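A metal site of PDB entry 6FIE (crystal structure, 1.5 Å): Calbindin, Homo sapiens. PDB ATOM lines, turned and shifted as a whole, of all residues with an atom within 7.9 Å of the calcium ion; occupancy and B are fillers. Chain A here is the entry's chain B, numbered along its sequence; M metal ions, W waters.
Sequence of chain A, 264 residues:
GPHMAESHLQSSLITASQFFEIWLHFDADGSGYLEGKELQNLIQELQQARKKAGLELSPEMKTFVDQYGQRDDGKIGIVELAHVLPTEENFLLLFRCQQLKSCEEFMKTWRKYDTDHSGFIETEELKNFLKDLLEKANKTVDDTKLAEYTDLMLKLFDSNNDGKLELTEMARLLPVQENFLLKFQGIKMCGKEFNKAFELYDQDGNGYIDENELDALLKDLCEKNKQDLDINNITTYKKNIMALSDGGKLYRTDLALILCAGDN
The backbone NH (N) of Asn 161 lies close to the side-chain carboxylate (OD1) of Asp 158, at 3.3 Å.
OD2 of Asp 158 is in hydrogen-bond range of N of Gly 163 (2.8 Å).
The backbone NH of Glu 166 sits close to the side-chain carboxylate of Glu 169, at 3.0 Å.
The side-chain carboxylate (OE2) of Glu 169 lies close to the backbone NH (N) of Ser 159 (3.3 Å).
Five residues have an atom within 4 Å of the calcium ion: Asp 158, Asn 160, Asp 162, Lys 164 and Glu 169.
Along chain A the residues within 4 Å of the calcium ion span positions 158 to 169.
The side-chain amide oxygen (OD1) of Asn 160 is bound to the calcium ion (2.3 Å).
OD1 of Asp 158 is bound to the calcium ion (2.3 Å).
The calcium ion is bound by OD1 of Asp 162 (2.3 Å).
Water W1 binds the calcium ion, 2.3 Å away.
O of Lys 164 binds the calcium ion, at 2.3 Å.
The calcium ion is bound by OE1 of Glu 169, 2.5 Å away.
The side-chain carboxylate (OE2) of Glu 169 binds the calcium ion, 2.6 Å away.
The calcium ion has seven donor atoms within binding distance.
Water W1 lies within hydrogen-bond range of OD2 of Asp 162, OE1 of Glu 166 and ND2 of Asn 160.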
ATOM      1  N   PHE A 120       7.827  17.143   3.274  1.00  0.00           N
ATOM      2  CA  PHE A 120       7.835  18.551   2.823  1.00  0.00           C
ATOM      3  C   PHE A 120       8.024  18.580   1.332  1.00  0.00           C
ATOM      4  O   PHE A 120       8.608  17.674   0.781  1.00  0.00           O
ATOM      5  CB  PHE A 120       8.984  19.357   3.397  1.00  0.00           C
ATOM      6  CG  PHE A 120       9.046  19.421   4.905  1.00  0.00           C
ATOM      7  CD1 PHE A 120       8.329  20.395   5.607  1.00  0.00           C
ATOM      8  CD2 PHE A 120       9.800  18.519   5.624  1.00  0.00           C
ATOM      9  CE1 PHE A 120       8.387  20.458   7.022  1.00  0.00           C
ATOM     10  CE2 PHE A 120       9.843  18.567   7.031  1.00  0.00           C
ATOM     11  CZ  PHE A 120       9.131  19.528   7.712  1.00  0.00           C
ATOM     12  N   ILE A 121       7.598  19.666   0.699  1.00  0.00           N
ATOM     13  CA  ILE A 121       7.879  19.935  -0.705  1.00  0.00           C
ATOM     14  C   ILE A 121       9.080  20.887  -0.748  1.00  0.00           C
ATOM     15  O   ILE A 121       8.958  22.077  -0.373  1.00  0.00           O
ATOM     16  CB  ILE A 121       6.640  20.449  -1.459  1.00  0.00           C
ATOM     17  CG1 ILE A 121       5.578  19.376  -1.586  1.00  0.00           C
ATOM     18  CG2 ILE A 121       7.017  21.044  -2.830  1.00  0.00           C
ATOM     19  CD1 ILE A 121       5.920  18.199  -2.497  1.00  0.00           C
ATOM     20  N   LEU A 154       7.884  29.830  -3.549  1.00  0.00           N
ATOM     21  CA  LEU A 154       8.381  29.411  -2.240  1.00  0.00           C
ATOM     22  C   LEU A 154       8.347  30.587  -1.262  1.00  0.00           C
ATOM     23  O   LEU A 154       7.794  30.461  -0.174  1.00  0.00           O
ATOM     24  CB  LEU A 154       9.789  28.858  -2.379  1.00  0.00           C
ATOM     25  CG  LEU A 154      10.406  28.346  -1.073  1.00  0.00           C
ATOM     26  CD1 LEU A 154       9.636  27.133  -0.540  1.00  0.00           C
ATOM     27  CD2 LEU A 154      11.860  27.985  -1.256  1.00  0.00           C
ATOM     28  N   PHE A 157       4.716  31.464  -0.148  1.00  0.00           N
ATOM     29  CA  PHE A 157       3.992  30.494   0.672  1.00  0.00           C
ATOM     30  C   PHE A 157       4.776  29.881   1.846  1.00  0.00           C
ATOM     31  O   PHE A 157       4.118  29.293   2.704  1.00  0.00           O
ATOM     32  CB  PHE A 157       3.428  29.379  -0.222  1.00  0.00           C
ATOM     33  CG  PHE A 157       2.267  29.846  -1.082  1.00  0.00           C
ATOM     34  CD1 PHE A 157       1.007  30.018  -0.530  1.00  0.00           C
ATOM     35  CD2 PHE A 157       2.479  30.348  -2.371  1.00  0.00           C
ATOM     36  CE1 PHE A 157      -0.047  30.553  -1.284  1.00  0.00           C
ATOM     37  CE2 PHE A 157       1.442  30.934  -3.090  1.00  0.00           C
ATOM     38  CZ  PHE A 157       0.192  31.029  -2.541  1.00  0.00           C
ATOM     39  N   ASP A 158       6.091  30.063   1.948  1.00  0.00           N
ATOM     40  CA  ASP A 158       6.908  29.490   3.032  1.00  0.00           C
ATOM     41  C   ASP A 158       6.776  30.346   4.302  1.00  0.00           C
ATOM     42  O   ASP A 158       7.701  31.064   4.648  1.00  0.00           O
ATOM     43  CB  ASP A 158       8.347  29.388   2.584  1.00  0.00           C
ATOM     44  CG  ASP A 158       9.297  28.849   3.621  1.00  0.00           C
ATOM     45  OD1 ASP A 158       8.808  28.205   4.586  1.00  0.00           O
ATOM     46  OD2 ASP A 158      10.531  28.984   3.419  1.00  0.00           O
ATOM     47  N   SER A 159       5.634  30.259   4.950  1.00  0.00           N
ATOM     48  CA  SER A 159       5.258  31.037   6.146  1.00  0.00           C
ATOM     49  C   SER A 159       6.297  31.012   7.261  1.00  0.00           C
ATOM     50  O   SER A 159       6.487  32.051   7.907  1.00  0.00           O
ATOM     51  CB  SER A 159       3.929  30.548   6.691  1.00  0.00           C
ATOM     52  OG  SER A 159       2.989  30.352   5.655  1.00  0.00           O
ATOM     53  N   ASN A 160       6.935  29.861   7.530  1.00  0.00           N
ATOM     54  CA  ASN A 160       7.923  29.807   8.613  1.00  0.00           C
ATOM     55  C   ASN A 160       9.354  30.050   8.176  1.00  0.00           C
ATOM     56  O   ASN A 160      10.260  29.892   8.985  1.00  0.00           O
ATOM     57  CB  ASN A 160       7.806  28.496   9.372  1.00  0.00           C
ATOM     58  CG  ASN A 160       8.330  27.297   8.632  1.00  0.00           C
ATOM     59  OD1 ASN A 160       8.479  27.313   7.395  1.00  0.00           O
ATOM     60  ND2 ASN A 160       8.561  26.205   9.356  1.00  0.00           N
ATOM     61  N   ASN A 161       9.590  30.375   6.894  1.00  0.00           N
ATOM     62  CA  ASN A 161      10.886  30.663   6.324  1.00  0.00           C
ATOM     63  C   ASN A 161      11.955  29.575   6.584  1.00  0.00           C
ATOM     64  O   ASN A 161      13.116  29.881   6.890  1.00  0.00           O
ATOM     65  CB  ASN A 161      11.369  32.079   6.756  1.00  0.00           C
ATOM     66  CG  ASN A 161      12.421  32.652   5.818  1.00  0.00           C
ATOM     67  OD1 ASN A 161      12.592  32.217   4.666  1.00  0.00           O
ATOM     68  ND2 ASN A 161      13.163  33.630   6.297  1.00  0.00           N
ATOM     69  N   ASP A 162      11.564  28.310   6.468  1.00  0.00           N
ATOM     70  CA  ASP A 162      12.526  27.194   6.592  1.00  0.00           C
ATOM     71  C   ASP A 162      13.067  26.716   5.202  1.00  0.00           C
ATOM     72  O   ASP A 162      13.831  25.764   5.142  1.00  0.00           O
ATOM     73  CB  ASP A 162      11.954  26.034   7.409  1.00  0.00           C
ATOM     74  CG  ASP A 162      10.793  25.298   6.803  1.00  0.00           C
ATOM     75  OD1 ASP A 162      10.291  25.740   5.728  1.00  0.00           O
ATOM     76  OD2 ASP A 162      10.293  24.341   7.443  1.00  0.00           O
ATOM     77  N   GLY A 163      12.660  27.389   4.120  1.00  0.00           N
ATOM     78  CA  GLY A 163      13.159  27.093   2.786  1.00  0.00           C
ATOM     79  C   GLY A 163      12.469  25.952   2.066  1.00  0.00           C
ATOM     80  O   GLY A 163      12.937  25.537   1.002  1.00  0.00           O
ATOM     81  N   LYS A 164      11.345  25.505   2.598  1.00  0.00           N
ATOM     82  CA  LYS A 164      10.547  24.399   2.039  1.00  0.00           C
ATOM     83  C   LYS A 164       9.103  24.525   2.486  1.00  0.00           C
ATOM     84  O   LYS A 164       8.791  25.255   3.433  1.00  0.00           O
ATOM     85  CB  LYS A 164      11.127  23.026   2.438  1.00  0.00           C
ATOM     86  CG  LYS A 164      11.135  22.782   3.943  1.00  0.00           C
ATOM     87  CD  LYS A 164      12.096  21.682   4.329  1.00  0.00           C
ATOM     88  CE  LYS A 164      12.121  21.559   5.832  1.00  0.00           C
ATOM     89  NZ  LYS A 164      13.024  20.462   6.278  1.00  0.00           N
ATOM     90  N   LEU A 165       8.184  23.859   1.770  1.00  0.00           N
ATOM     91  CA  LEU A 165       6.779  23.947   2.043  1.00  0.00           C
ATOM     92  C   LEU A 165       6.294  22.757   2.819  1.00  0.00           C
ATOM     93  O   LEU A 165       6.585  21.643   2.413  1.00  0.00           O
ATOM     94  CB  LEU A 165       5.952  24.074   0.745  1.00  0.00           C
ATOM     95  CG  LEU A 165       6.280  25.309  -0.094  1.00  0.00           C
ATOM     96  CD1 LEU A 165       5.449  25.343  -1.405  1.00  0.00           C
ATOM     97  CD2 LEU A 165       6.036  26.592   0.694  1.00  0.00           C
ATOM     98  N   GLU A 166       5.474  22.970   3.853  1.00  0.00           N
ATOM     99  CA  GLU A 166       4.766  21.949   4.591  1.00  0.00           C
ATOM    100  C   GLU A 166       3.319  21.989   4.074  1.00  0.00           C
ATOM    101  O   GLU A 166       2.886  22.947   3.416  1.00  0.00           O
ATOM    102  CB  GLU A 166       4.886  22.105   6.108  1.00  0.00           C
ATOM    103  CG  GLU A 166       4.294  23.374   6.698  1.00  0.00           C
ATOM    104  CD  GLU A 166       4.518  23.404   8.191  1.00  0.00           C
ATOM    105  OE1 GLU A 166       5.649  23.762   8.600  1.00  0.00           O
ATOM    106  OE2 GLU A 166       3.651  22.872   8.924  1.00  0.00           O
ATOM    107  N   LEU A 167       2.587  20.947   4.336  1.00  0.00           N
ATOM    108  CA  LEU A 167       1.246  20.762   3.813  1.00  0.00           C
ATOM    109  C   LEU A 167       0.344  21.970   4.067  1.00  0.00           C
ATOM    110  O   LEU A 167      -0.338  22.398   3.148  1.00  0.00           O
ATOM    111  CB  LEU A 167       0.590  19.498   4.385  1.00  0.00           C
ATOM    112  CG  LEU A 167      -0.774  19.153   3.829  1.00  0.00           C
ATOM    113  CD1 LEU A 167      -0.675  18.712   2.395  1.00  0.00           C
ATOM    114  CD2 LEU A 167      -1.409  18.054   4.611  1.00  0.00           C
ATOM    115  N   GLU A 169       1.152  25.072   4.563  1.00  0.00           N
ATOM    116  CA  GLU A 169       1.609  26.232   3.786  1.00  0.00           C
ATOM    117  C   GLU A 169       1.128  26.168   2.343  1.00  0.00           C
ATOM    118  O   GLU A 169       0.488  27.099   1.839  1.00  0.00           O
ATOM    119  CB  GLU A 169       3.101  26.358   3.797  1.00  0.00           C
ATOM    120  CG  GLU A 169       3.663  26.787   5.130  1.00  0.00           C
ATOM    121  CD  GLU A 169       5.169  26.644   5.221  1.00  0.00           C
ATOM    122  OE1 GLU A 169       5.776  25.933   4.389  1.00  0.00           O
ATOM    123  OE2 GLU A 169       5.750  27.238   6.160  1.00  0.00           O
ATOM    124  N   MET A 170       1.435  25.053   1.655  1.00  0.00           N
ATOM    125  CA  MET A 170       0.985  24.870   0.282  1.00  0.00           C
ATOM    126  C   MET A 170      -0.544  24.805   0.124  1.00  0.00           C
ATOM    127  O   MET A 170      -1.054  25.225  -0.930  1.00  0.00           O
ATOM    128  CB  MET A 170       1.630  23.610  -0.332  1.00  0.00           C
ATOM    129  CG  MET A 170       1.636  23.637  -1.809  1.00  0.00           C
ATOM    130  SD  MET A 170       2.526  22.197  -2.433  1.00  0.00           S
ATOM    131  CE  MET A 170       2.534  22.562  -4.175  1.00  0.00           C
HETATM  132 CA    CA M   1       8.048  26.202   5.432  1.00  0.00          CA
HETATM  133  O   HOH W   1       7.736  24.231   6.599  1.00  0.00           O
